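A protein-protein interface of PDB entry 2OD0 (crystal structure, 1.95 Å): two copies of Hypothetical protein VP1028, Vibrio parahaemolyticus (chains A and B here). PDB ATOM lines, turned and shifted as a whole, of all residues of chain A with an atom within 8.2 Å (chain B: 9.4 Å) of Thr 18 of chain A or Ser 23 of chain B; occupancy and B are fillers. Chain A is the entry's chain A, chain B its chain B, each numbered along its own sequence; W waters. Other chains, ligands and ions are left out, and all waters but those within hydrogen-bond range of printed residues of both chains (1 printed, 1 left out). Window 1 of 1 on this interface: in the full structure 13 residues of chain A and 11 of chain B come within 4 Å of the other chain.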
ATOM      1  N   MET A  10      22.662   6.262 -15.025  1.00  0.00           N
ATOM      2  CA  MET A  10      24.001   6.808 -15.223  1.00  0.00           C
ATOM      3  C   MET A  10      24.734   5.964 -16.230  1.00  0.00           C
ATOM      4  O   MET A  10      25.316   6.489 -17.164  1.00  0.00           O
ATOM      5  CB  MET A  10      24.748   6.883 -13.902  1.00  0.00           C
ATOM      6  CG  MET A  10      24.158   7.905 -12.991  1.00  0.00           C
ATOM      7  SD  MET A  10      25.155   8.079 -11.308  1.00  0.00           S
ATOM      8  CE  MET A  10      26.758   8.981 -12.032  1.00  0.00           C
ATOM      9  N   LYS A  11      24.606   4.642 -16.116  1.00  0.00           N
ATOM     10  CA  LYS A  11      25.291   3.754 -17.066  1.00  0.00           C
ATOM     11  C   LYS A  11      24.751   3.944 -18.494  1.00  0.00           C
ATOM     12  O   LYS A  11      25.531   4.044 -19.449  1.00  0.00           O
ATOM     13  CB  LYS A  11      25.212   2.298 -16.610  1.00  0.00           C
ATOM     14  CG  LYS A  11      25.739   1.276 -17.605  1.00  0.00           C
ATOM     15  CD  LYS A  11      26.059  -0.060 -16.902  1.00  0.00           C
ATOM     16  CE  LYS A  11      25.638  -1.331 -17.724  1.00  0.00           C
ATOM     17  NZ  LYS A  11      26.557  -2.489 -17.431  1.00  0.00           N
ATOM     18  N   PHE A  13      23.344   6.514 -19.848  1.00  0.00           N
ATOM     19  CA  PHE A  13      23.674   7.821 -20.411  1.00  0.00           C
ATOM     20  C   PHE A  13      25.153   8.118 -20.626  1.00  0.00           C
ATOM     21  O   PHE A  13      25.489   9.195 -21.131  1.00  0.00           O
ATOM     22  CB  PHE A  13      22.985   8.920 -19.612  1.00  0.00           C
ATOM     23  CG  PHE A  13      21.480   8.825 -19.655  1.00  0.00           C
ATOM     24  CD1 PHE A  13      20.807   8.633 -20.872  1.00  0.00           C
ATOM     25  CD2 PHE A  13      20.728   8.916 -18.506  1.00  0.00           C
ATOM     26  CE1 PHE A  13      19.417   8.547 -20.940  1.00  0.00           C
ATOM     27  CE2 PHE A  13      19.285   8.828 -18.574  1.00  0.00           C
ATOM     28  CZ  PHE A  13      18.652   8.629 -19.799  1.00  0.00           C
ATOM     29  N   GLU A  14      26.019   7.160 -20.307  1.00  0.00           N
ATOM     30  CA  GLU A  14      27.426   7.235 -20.708  1.00  0.00           C
ATOM     31  C   GLU A  14      27.608   7.343 -22.236  1.00  0.00           C
ATOM     32  O   GLU A  14      28.663   7.744 -22.698  1.00  0.00           O
ATOM     33  CB  GLU A  14      28.231   6.071 -20.105  1.00  0.00           C
ATOM     34  CG  GLU A  14      28.431   6.260 -18.601  1.00  0.00           C
ATOM     35  CD  GLU A  14      29.223   5.173 -17.938  1.00  0.00           C
ATOM     36  OE1 GLU A  14      29.392   4.098 -18.546  1.00  0.00           O
ATOM     37  OE2 GLU A  14      29.678   5.399 -16.789  1.00  0.00           O
ATOM     38  N   ALA A  15      26.564   7.034 -23.011  1.00  0.00           N
ATOM     39  CA  ALA A  15      26.493   7.418 -24.417  1.00  0.00           C
ATOM     40  C   ALA A  15      26.688   8.914 -24.627  1.00  0.00           C
ATOM     41  O   ALA A  15      27.050   9.335 -25.713  1.00  0.00           O
ATOM     42  CB  ALA A  15      25.130   6.971 -25.045  1.00  0.00           C
ATOM     43  N   LEU A  16      26.459   9.719 -23.595  1.00  0.00           N
ATOM     44  CA  LEU A  16      26.683  11.161 -23.657  1.00  0.00           C
ATOM     45  C   LEU A  16      28.058  11.586 -23.112  1.00  0.00           C
ATOM     46  O   LEU A  16      28.363  12.787 -23.042  1.00  0.00           O
ATOM     47  CB  LEU A  16      25.580  11.898 -22.873  1.00  0.00           C
ATOM     48  CG  LEU A  16      24.156  11.964 -23.447  1.00  0.00           C
ATOM     49  CD1 LEU A  16      23.584  10.597 -23.803  1.00  0.00           C
ATOM     50  CD2 LEU A  16      23.259  12.695 -22.447  1.00  0.00           C
ATOM     51  N   GLY A  17      28.873  10.607 -22.737  1.00  0.00           N
ATOM     52  CA  GLY A  17      30.166  10.842 -22.116  1.00  0.00           C
ATOM     53  C   GLY A  17      30.109  10.584 -20.633  1.00  0.00           C
ATOM     54  O   GLY A  17      29.169   9.985 -20.138  1.00  0.00           O
ATOM     55  N   THR A  18      31.102  11.072 -19.906  1.00  0.00           N
ATOM     56  CA  THR A  18      31.123  10.901 -18.458  1.00  0.00           C
ATOM     57  C   THR A  18      29.837  11.465 -17.835  1.00  0.00           C
ATOM     58  O   THR A  18      29.408  12.572 -18.162  1.00  0.00           O
ATOM     59  CB  THR A  18      32.331  11.618 -17.854  1.00  0.00           C
ATOM     60  OG1 THR A  18      33.535  11.050 -18.408  1.00  0.00           O
ATOM     61  CG2 THR A  18      32.332  11.524 -16.303  1.00  0.00           C
ATOM     62  N   ILE A  19      29.245  10.709 -16.920  1.00  0.00           N
ATOM     63  CA  ILE A  19      28.038  11.148 -16.214  1.00  0.00           C
ATOM     64  C   ILE A  19      28.437  11.379 -14.771  1.00  0.00           C
ATOM     65  O   ILE A  19      29.148  10.544 -14.177  1.00  0.00           O
ATOM     66  CB  ILE A  19      26.880  10.125 -16.340  1.00  0.00           C
ATOM     67  CG1 ILE A  19      26.521   9.904 -17.811  1.00  0.00           C
ATOM     68  CG2 ILE A  19      25.635  10.578 -15.549  1.00  0.00           C
ATOM     69  CD1 ILE A  19      26.141  11.177 -18.584  1.00  0.00           C
ATOM     70  N   LYS A  20      28.027  12.537 -14.247  1.00  0.00           N
ATOM     71  CA  LYS A  20      28.247  12.920 -12.861  1.00  0.00           C
ATOM     72  C   LYS A  20      26.914  13.072 -12.155  1.00  0.00           C
ATOM     73  O   LYS A  20      25.921  13.400 -12.792  1.00  0.00           O
ATOM     74  CB  LYS A  20      29.037  14.219 -12.787  1.00  0.00           C
ATOM     75  CG  LYS A  20      30.399  14.111 -13.488  1.00  0.00           C
ATOM     76  CD  LYS A  20      31.219  15.348 -13.389  1.00  0.00           C
ATOM     77  CE  LYS A  20      32.608  15.113 -14.019  1.00  0.00           C
ATOM     78  NZ  LYS A  20      33.398  16.362 -13.888  1.00  0.00           N
ATOM     79  N   SER A  21      26.899  12.793 -10.858  1.00  0.00           N
ATOM     80  CA  SER A  21      25.689  12.921 -10.043  1.00  0.00           C
ATOM     81  C   SER A  21      26.012  13.629  -8.724  1.00  0.00           C
ATOM     82  O   SER A  21      27.144  13.514  -8.193  1.00  0.00           O
ATOM     83  CB  SER A  21      25.069  11.571  -9.756  1.00  0.00           C
ATOM     84  OG  SER A  21      23.806  11.719  -9.140  1.00  0.00           O
ATOM     85  N   LEU A  30      21.550  14.172 -12.680  1.00  0.00           N
ATOM     86  CA  LEU A  30      22.498  13.591 -13.617  1.00  0.00           C
ATOM     87  C   LEU A  30      23.004  14.701 -14.544  1.00  0.00           C
ATOM     88  O   LEU A  30      22.216  15.468 -15.077  1.00  0.00           O
ATOM     89  CB  LEU A  30      21.872  12.451 -14.441  1.00  0.00           C
ATOM     90  CG  LEU A  30      21.522  11.110 -13.764  1.00  0.00           C
ATOM     91  CD1 LEU A  30      20.441  11.230 -12.791  1.00  0.00           C
ATOM     92  CD2 LEU A  30      21.136  10.032 -14.823  1.00  0.00           C
ATOM     93  N   PHE A  31      24.326  14.746 -14.707  1.00  0.00           N
ATOM     94  CA  PHE A  31      25.049  15.803 -15.424  1.00  0.00           C
ATOM     95  C   PHE A  31      25.974  15.206 -16.477  1.00  0.00           C
ATOM     96  O   PHE A  31      26.647  14.200 -16.232  1.00  0.00           O
ATOM     97  CB  PHE A  31      25.927  16.615 -14.466  1.00  0.00           C
ATOM     98  CG  PHE A  31      25.187  17.309 -13.392  1.00  0.00           C
ATOM     99  CD1 PHE A  31      25.053  18.678 -13.406  1.00  0.00           C
ATOM    100  CD2 PHE A  31      24.660  16.607 -12.323  1.00  0.00           C
ATOM    101  CE1 PHE A  31      24.396  19.320 -12.388  1.00  0.00           C
ATOM    102  CE2 PHE A  31      23.963  17.273 -11.298  1.00  0.00           C
ATOM    103  CZ  PHE A  31      23.841  18.601 -11.331  1.00  0.00           C
ATOM    104  N   ALA A  32      25.978  15.841 -17.647  1.00  0.00           N
ATOM    105  CA  ALA A  32      26.903  15.551 -18.728  1.00  0.00           C
ATOM    106  C   ALA A  32      27.388  16.896 -19.219  1.00  0.00           C
ATOM    107  O   ALA A  32      26.630  17.868 -19.211  1.00  0.00           O
ATOM    108  CB  ALA A  32      26.200  14.791 -19.833  1.00  0.00           C
ATOM    109  N   ASP A  33      28.657  16.981 -19.605  1.00  0.00           N
ATOM    110  CA  ASP A  33      29.237  18.241 -20.035  1.00  0.00           C
ATOM    111  C   ASP A  33      28.867  19.383 -19.081  1.00  0.00           C
ATOM    112  O   ASP A  33      28.492  20.461 -19.535  1.00  0.00           O
ATOM    113  CB  ASP A  33      28.738  18.562 -21.446  1.00  0.00           C
ATOM    114  CG  ASP A  33      29.021  17.445 -22.439  1.00  0.00           C
ATOM    115  OD1 ASP A  33      30.088  16.783 -22.330  1.00  0.00           O
ATOM    116  OD2 ASP A  33      28.197  17.259 -23.358  1.00  0.00           O
ATOM    117  N   GLU A  34      28.931  19.124 -17.773  1.00  0.00           N
ATOM    118  CA  GLU A  34      28.621  20.123 -16.718  1.00  0.00           C
ATOM    119  C   GLU A  34      27.194  20.649 -16.704  1.00  0.00           C
ATOM    120  O   GLU A  34      26.950  21.710 -16.143  1.00  0.00           O
ATOM    121  CB  GLU A  34      29.566  21.333 -16.798  1.00  0.00           C
ATOM    122  CG  GLU A  34      31.016  20.991 -16.640  1.00  0.00           C
ATOM    123  CD  GLU A  34      31.913  22.209 -16.356  1.00  0.00           C
ATOM    124  OE1 GLU A  34      31.556  23.376 -16.704  1.00  0.00           O
ATOM    125  OE2 GLU A  34      33.010  21.986 -15.782  1.00  0.00           O
ATOM    126  N   THR A  35      26.260  19.939 -17.326  1.00  0.00           N
ATOM    127  CA  THR A  35      24.873  20.390 -17.442  1.00  0.00           C
ATOM    128  C   THR A  35      23.936  19.291 -16.981  1.00  0.00           C
ATOM    129  O   THR A  35      24.027  18.170 -17.468  1.00  0.00           O
ATOM    130  CB  THR A  35      24.530  20.719 -18.892  1.00  0.00           C
ATOM    131  OG1 THR A  35      25.435  21.715 -19.347  1.00  0.00           O
ATOM    132  CG2 THR A  35      23.109  21.254 -19.027  1.00  0.00           C
ATOM    133  N   PHE A  37      20.656  17.172 -16.876  1.00  0.00           N
ATOM    134  CA  PHE A  37      19.643  16.808 -17.859  1.00  0.00           C
ATOM    135  C   PHE A  37      18.601  15.809 -17.321  1.00  0.00           C
ATOM    136  O   PHE A  37      17.607  15.520 -17.990  1.00  0.00           O
ATOM    137  CB  PHE A  37      20.308  16.258 -19.144  1.00  0.00           C
ATOM    138  CG  PHE A  37      21.002  14.958 -18.937  1.00  0.00           C
ATOM    139  CD1 PHE A  37      22.299  14.924 -18.437  1.00  0.00           C
ATOM    140  CD2 PHE A  37      20.347  13.755 -19.199  1.00  0.00           C
ATOM    141  CE1 PHE A  37      22.931  13.706 -18.189  1.00  0.00           C
ATOM    142  CE2 PHE A  37      20.970  12.533 -18.966  1.00  0.00           C
ATOM    143  CZ  PHE A  37      22.254  12.500 -18.461  1.00  0.00           C
ATOM    144  N   LEU A 100      19.712  17.596 -22.995  1.00  0.00           N
ATOM    145  CA  LEU A 100      21.011  18.223 -22.764  1.00  0.00           C
ATOM    146  C   LEU A 100      21.248  19.363 -23.776  1.00  0.00           C
ATOM    147  O   LEU A 100      21.698  20.445 -23.418  1.00  0.00           O
ATOM    148  CB  LEU A 100      22.127  17.176 -22.876  1.00  0.00           C
ATOM    149  CG  LEU A 100      23.563  17.580 -22.514  1.00  0.00           C
ATOM    150  CD1 LEU A 100      23.681  17.925 -21.019  1.00  0.00           C
ATOM    151  CD2 LEU A 100      24.527  16.481 -22.902  1.00  0.00           C
ATOM    152  N   LEU B   6      24.583   1.917  -5.264  1.00  0.00           N
ATOM    153  CA  LEU B   6      25.139   3.246  -5.508  1.00  0.00           C
ATOM    154  C   LEU B   6      24.356   4.313  -4.767  1.00  0.00           C
ATOM    155  O   LEU B   6      24.919   5.147  -4.044  1.00  0.00           O
ATOM    156  CB  LEU B   6      25.193   3.578  -7.024  1.00  0.00           C
ATOM    157  CG  LEU B   6      25.721   4.983  -7.381  1.00  0.00           C
ATOM    158  CD1 LEU B   6      27.153   5.178  -6.916  1.00  0.00           C
ATOM    159  CD2 LEU B   6      25.623   5.299  -8.887  1.00  0.00           C
ATOM    160  N   LYS B  20      29.469  13.203  -4.141  1.00  0.00           N
ATOM    161  CA  LYS B  20      29.228  13.200  -5.580  1.00  0.00           C
ATOM    162  C   LYS B  20      29.702  11.892  -6.190  1.00  0.00           C
ATOM    163  O   LYS B  20      30.613  11.250  -5.665  1.00  0.00           O
ATOM    164  CB  LYS B  20      29.989  14.353  -6.243  1.00  0.00           C
ATOM    165  CG  LYS B  20      29.560  15.712  -5.747  1.00  0.00           C
ATOM    166  CD  LYS B  20      30.341  16.812  -6.430  1.00  0.00           C
ATOM    167  CE  LYS B  20      29.732  18.195  -6.135  1.00  0.00           C
ATOM    168  NZ  LYS B  20      30.650  19.248  -6.665  1.00  0.00           N
ATOM    169  N   SER B  21      29.103  11.505  -7.309  1.00  0.00           N
ATOM    170  CA  SER B  21      29.564  10.333  -8.049  1.00  0.00           C
ATOM    171  C   SER B  21      29.790  10.614  -9.532  1.00  0.00           C
ATOM    172  O   SER B  21      29.260  11.579 -10.109  1.00  0.00           O
ATOM    173  CB  SER B  21      28.651   9.125  -7.867  1.00  0.00           C
ATOM    174  OG  SER B  21      27.360   9.331  -8.405  1.00  0.00           O
ATOM    175  N   ARG B  22      30.608   9.781 -10.155  1.00  0.00           N
ATOM    176  CA  ARG B  22      30.831   9.893 -11.576  1.00  0.00           C
ATOM    177  C   ARG B  22      31.344   8.586 -12.158  1.00  0.00           C
ATOM    178  O   ARG B  22      31.824   7.702 -11.419  1.00  0.00           O
ATOM    179  CB  ARG B  22      31.806  11.021 -11.891  1.00  0.00           C
ATOM    180  CG  ARG B  22      33.192  10.877 -11.287  1.00  0.00           C
ATOM    181  CD  ARG B  22      34.243  11.613 -12.119  1.00  0.00           C
ATOM    182  NE  ARG B  22      34.503  10.882 -13.356  1.00  0.00           N
ATOM    183  CZ  ARG B  22      35.286  11.300 -14.357  1.00  0.00           C
ATOM    184  NH1 ARG B  22      35.465  10.518 -15.430  1.00  0.00           N
ATOM    185  NH2 ARG B  22      35.897  12.478 -14.290  1.00  0.00           N
ATOM    186  N   SER B  23      31.186   8.464 -13.471  1.00  0.00           N
ATOM    187  CA  SER B  23      31.720   7.338 -14.225  1.00  0.00           C
ATOM    188  C   SER B  23      33.196   7.212 -13.842  1.00  0.00           C
ATOM    189  O   SER B  23      33.948   8.152 -13.995  1.00  0.00           O
ATOM    190  CB  SER B  23      31.619   7.598 -15.739  1.00  0.00           C
ATOM    191  OG  SER B  23      30.297   7.899 -16.160  1.00  0.00           O
ATOM    192  N   MET B  24      33.594   6.071 -13.301  1.00  0.00           N
ATOM    193  CA  MET B  24      35.025   5.799 -13.003  1.00  0.00           C
ATOM    194  C   MET B  24      35.333   4.349 -13.119  1.00  0.00           C
ATOM    195  O   MET B  24      34.695   3.522 -12.476  1.00  0.00           O
ATOM    196  CB  MET B  24      35.428   6.189 -11.575  1.00  0.00           C
ATOM    197  CG  MET B  24      35.472   7.644 -11.240  1.00  0.00           C
ATOM    198  SD  MET B  24      36.837   8.704 -12.218  1.00  0.00           S
ATOM    199  CE  MET B  24      38.480   8.123 -11.336  1.00  0.00           C
ATOM    200  N   PHE B  25      36.367   4.033 -13.896  1.00  0.00           N
ATOM    201  CA  PHE B  25      36.917   2.682 -13.967  1.00  0.00           C
ATOM    202  C   PHE B  25      35.900   1.619 -14.276  1.00  0.00           C
ATOM    203  O   PHE B  25      36.021   0.485 -13.818  1.00  0.00           O
ATOM    204  CB  PHE B  25      37.635   2.291 -12.674  1.00  0.00           C
ATOM    205  CG  PHE B  25      38.581   3.322 -12.179  1.00  0.00           C
ATOM    206  CD1 PHE B  25      39.357   4.069 -13.066  1.00  0.00           C
ATOM    207  CD2 PHE B  25      38.691   3.567 -10.820  1.00  0.00           C
ATOM    208  CE1 PHE B  25      40.228   5.053 -12.597  1.00  0.00           C
ATOM    209  CE2 PHE B  25      39.562   4.534 -10.346  1.00  0.00           C
ATOM    210  CZ  PHE B  25      40.338   5.269 -11.234  1.00  0.00           C
ATOM    211  N   GLY B  26      34.912   1.960 -15.076  1.00  0.00           N
ATOM    212  CA  GLY B  26      33.930   0.967 -15.507  1.00  0.00           C
ATOM    213  C   GLY B  26      32.753   0.897 -14.546  1.00  0.00           C
ATOM    214  O   GLY B  26      31.801   0.190 -14.792  1.00  0.00           O
ATOM    215  N   GLY B  27      32.817   1.649 -13.451  1.00  0.00           N
ATOM    216  CA  GLY B  27      31.725   1.727 -12.502  1.00  0.00           C
ATOM    217  C   GLY B  27      31.450   3.180 -12.137  1.00  0.00           C
ATOM    218  O   GLY B  27      31.545   4.077 -12.983  1.00  0.00           O
ATOM    219  N   PHE B  28      31.087   3.412 -10.881  1.00  0.00           N
ATOM    220  CA  PHE B  28      30.840   4.771 -10.391  1.00  0.00           C
ATOM    221  C   PHE B  28      31.626   5.074  -9.143  1.00  0.00           C
ATOM    222  O   PHE B  28      31.468   4.394  -8.109  1.00  0.00           O
ATOM    223  CB  PHE B  28      29.331   5.021 -10.215  1.00  0.00           C
ATOM    224  CG  PHE B  28      28.629   4.964 -11.490  1.00  0.00           C
ATOM    225  CD1 PHE B  28      28.730   6.021 -12.372  1.00  0.00           C
ATOM    226  CD2 PHE B  28      28.034   3.811 -11.902  1.00  0.00           C
ATOM    227  CE1 PHE B  28      28.187   5.942 -13.605  1.00  0.00           C
ATOM    228  CE2 PHE B  28      27.480   3.729 -13.153  1.00  0.00           C
ATOM    229  CZ  PHE B  28      27.548   4.795 -14.003  1.00  0.00           C
ATOM    230  N   GLY B  29      32.472   6.084  -9.254  1.00  0.00           N
ATOM    231  CA  GLY B  29      33.294   6.539  -8.146  1.00  0.00           C
ATOM    232  C   GLY B  29      32.515   7.482  -7.258  1.00  0.00           C
ATOM    233  O   GLY B  29      31.716   8.278  -7.742  1.00  0.00           O
ATOM    234  N   LEU B  30      32.739   7.364  -5.958  1.00  0.00           N
ATOM    235  CA  LEU B  30      32.152   8.204  -4.942  1.00  0.00           C
ATOM    236  C   LEU B  30      33.251   9.101  -4.383  1.00  0.00           C
ATOM    237  O   LEU B  30      34.317   8.628  -3.943  1.00  0.00           O
ATOM    238  CB  LEU B  30      31.533   7.357  -3.805  1.00  0.00           C
ATOM    239  CG  LEU B  30      30.236   6.598  -4.115  1.00  0.00           C
ATOM    240  CD1 LEU B  30      30.452   5.377  -4.934  1.00  0.00           C
ATOM    241  CD2 LEU B  30      29.511   6.194  -2.836  1.00  0.00           C
ATOM    242  N   PHE B  31      32.940  10.391  -4.362  1.00  0.00           N
ATOM    243  CA  PHE B  31      33.840  11.446  -3.931  1.00  0.00           C
ATOM    244  C   PHE B  31      33.236  12.189  -2.756  1.00  0.00           C
ATOM    245  O   PHE B  31      32.031  12.509  -2.762  1.00  0.00           O
ATOM    246  CB  PHE B  31      34.018  12.456  -5.075  1.00  0.00           C
ATOM    247  CG  PHE B  31      34.710  11.893  -6.275  1.00  0.00           C
ATOM    248  CD1 PHE B  31      35.971  12.339  -6.631  1.00  0.00           C
ATOM    249  CD2 PHE B  31      34.099  10.939  -7.064  1.00  0.00           C
ATOM    250  CE1 PHE B  31      36.617  11.853  -7.751  1.00  0.00           C
ATOM    251  CE2 PHE B  31      34.741  10.436  -8.176  1.00  0.00           C
ATOM    252  CZ  PHE B  31      36.006  10.907  -8.524  1.00  0.00           C
ATOM    253  N   MET B  36      37.977  10.947  -4.181  1.00  0.00           N
ATOM    254  CA  MET B  36      37.403   9.616  -4.334  1.00  0.00           C
ATOM    255  C   MET B  36      37.857   8.653  -3.214  1.00  0.00           C
ATOM    256  O   MET B  36      39.041   8.566  -2.857  1.00  0.00           O
ATOM    257  CB  MET B  36      37.746   9.048  -5.699  1.00  0.00           C
ATOM    258  CG  MET B  36      36.926   7.843  -6.067  1.00  0.00           C
ATOM    259  SD  MET B  36      37.306   7.302  -7.910  1.00  0.00           S
ATOM    260  CE  MET B  36      36.865   5.400  -7.788  1.00  0.00           C
ATOM    261  N   ALA B  38      35.587   5.549  -2.748  1.00  0.00           N
ATOM    262  CA  ALA B  38      34.818   4.329  -2.957  1.00  0.00           C
ATOM    263  C   ALA B  38      34.445   4.187  -4.412  1.00  0.00           C
ATOM    264  O   ALA B  38      34.527   5.134  -5.190  1.00  0.00           O
ATOM    265  CB  ALA B  38      33.559   4.279  -2.023  1.00  0.00           C
ATOM    266  N   LEU B  39      34.081   2.971  -4.784  1.00  0.00           N
ATOM    267  CA  LEU B  39      33.700   2.633  -6.147  1.00  0.00           C
ATOM    268  C   LEU B  39      32.627   1.567  -6.118  1.00  0.00           C
ATOM    269  O   LEU B  39      32.788   0.510  -5.475  1.00  0.00           O
ATOM    270  CB  LEU B  39      34.949   2.142  -6.932  1.00  0.00           C
ATOM    271  CG  LEU B  39      34.790   1.557  -8.336  1.00  0.00           C
ATOM    272  CD1 LEU B  39      34.396   2.677  -9.421  1.00  0.00           C
ATOM    273  CD2 LEU B  39      36.064   0.785  -8.738  1.00  0.00           C
ATOM    274  N   VAL B  40      31.530   1.835  -6.813  1.00  0.00           N
ATOM    275  CA  VAL B  40      30.515   0.845  -7.048  1.00  0.00           C
ATOM    276  C   VAL B  40      30.661   0.262  -8.441  1.00  0.00           C
ATOM    277  O   VAL B  40      30.613   0.990  -9.429  1.00  0.00           O
ATOM    278  CB  VAL B  40      29.099   1.430  -6.915  1.00  0.00           C
ATOM    279  CG1 VAL B  40      28.085   0.320  -7.185  1.00  0.00           C
ATOM    280  CG2 VAL B  40      28.903   2.033  -5.507  1.00  0.00           C
ATOM    281  N   TYR B  67      39.777  -3.007 -13.891  1.00  0.00           N
ATOM    282  CA  TYR B  67      38.953  -2.517 -15.001  1.00  0.00           C
ATOM    283  C   TYR B  67      39.564  -2.973 -16.329  1.00  0.00           C
ATOM    284  O   TYR B  67      40.773  -2.808 -16.542  1.00  0.00           O
ATOM    285  CB  TYR B  67      38.880  -0.988 -14.884  1.00  0.00           C
ATOM    286  CG  TYR B  67      38.453  -0.198 -16.099  1.00  0.00           C
ATOM    287  CD1 TYR B  67      37.325  -0.529 -16.821  1.00  0.00           C
ATOM    288  CD2 TYR B  67      39.183   0.918 -16.488  1.00  0.00           C
ATOM    289  CE1 TYR B  67      36.919   0.224 -17.929  1.00  0.00           C
ATOM    290  CE2 TYR B  67      38.807   1.661 -17.567  1.00  0.00           C
ATOM    291  CZ  TYR B  67      37.659   1.315 -18.291  1.00  0.00           C
ATOM    292  OH  TYR B  67      37.296   2.091 -19.371  1.00  0.00           O
HETATM  293  O   HOH W   1      30.678   1.776 -17.656  1.00  0.00           O
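The backbone NH of Ser 21 of chain A sits at hydrogen-bond distance from the backbone carbonyl oxygen of Ser 21 of chain B (2.8 Å). The side-chain carboxylate (OE2) of Glu 14 of chain A sits at hydrogen-bond distance from the side-chain hydroxyl (OG) of Ser 23 of chain B (2.7 Å). O of Ile 19 of chain A is in hydrogen-bond range of N of Ser 23 of chain B, at 3.0 Å.
The backbone carbonyl oxygen (O) of Lys 20 of chain A lies within hydrogen-bond range of the backbone NH (N) of Phe 31 of chain A, 2.8 Å away. The backbone carbonyl oxygen of Val 40 of chain B sits at hydrogen-bond distance from the backbone NH of Phe 28 of chain B (2.9 Å). The backbone carbonyl oxygen (O) of Arg 22 of chain B lies within hydrogen-bond range of the backbone NH (N) of Gly 29 of chain B (2.8 Å). The guanidinium group of Arg 22 of chain B is in hydrogen-bond range of the side-chain sulfur of Met 24 of chain B (3.4 Å). The backbone carbonyl oxygen (O) of Lys 20 of chain B is in hydrogen-bond range of the backbone NH (N) of Phe 31 of chain B, at 2.8 Å.
Leu 6 of chain B touches Met 10 of chain A. CE of Met 10 of chain A touches OG of Ser 21 of chain B, at 3.7 Å. CB of Met 10 of chain A touches CZ of Phe 28 of chain B, at 3.5 Å. Lys 11 of chain A touches Phe 28 of chain B. Glu 14 of chain A touches Phe 28 of chain B. Thr 18 of chain A touches Ser 23 of chain B (CA to OG, 3.9 Å). Ile 19 of chain A touches Arg 22 of chain B. Ser 21 of chain B touches Lys 20 of chain A (O to CA, 3.2 Å). Arg 22 of chain B touches Lys 20 of chain A. Ser 21 of chain A touches Lys 20 of chain B (O to CA, 3.4 Å).
Of chain B, only Arg 22 (3.4 Å) and Ser 23 (3.9 Å) come within 4 Å of Thr 18 of chain A. Of chain A, only Glu 14 (2.7 Å), Thr 18 (3.9 Å) and Ile 19 (3.0 Å) come within 4 Å of Ser 23 of chain B. Of chain B, only Arg 22 (3.2 Å) and Ser 23 (3.0 Å) come within 4 Å of Ile 19 of chain A. Printed residues of chain B within 4 Å of Met 10 of chain A: Leu 6, Ser 21 and Phe 28. Of the printed residues of chain A, Arg 22 of chain B touches Thr 18, Ile 19 and Lys 20. Printed residues of chain A within 4 Å of Leu 6 of chain B: Met 10. Phe 31 of chain A touches none of the printed residues of chain B. The nearest residue of chain B that does not touch Thr 18 of chain A is Met 24 of chain B (6.4 Å).
Of the 18 printed residues of chain B, 6 touch a printed residue of chain A. Printed residues of chain B that touch a printed residue of chain A: Leu 6, Lys 20, Ser 21, Arg 22, Ser 23 and Phe 28. Of the 19 printed residues of chain A, 7 touch a printed residue of chain B. Printed residues of chain A that touch a printed residue of chain B: Met 10, Lys 11, Glu 14, Thr 18, Ile 19, Lys 20 and Ser 21. Hydrophobic or aromatic side chains of chain A within 4 Å of the printed part of chain B: Met 10. Among the printed residues, 14 pairs touch across the chains. Among the printed residues, no Asp or Glu carboxylate lies within 4 Å of a Lys or Arg side-chain nitrogen of the other chain.
Lys 20 of chain A touches Ser 21 of chain B, and with the chains exchanged Ser 21 of chain A touches Lys 20 of chain B. Ser 21 of chain A touches its own counterpart, Ser 21 of chain B.
Water W1 bridges OE1 of Glu 14 of chain A (2.8 Å) and O of Gly 26 of chain B (3.5 Å).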
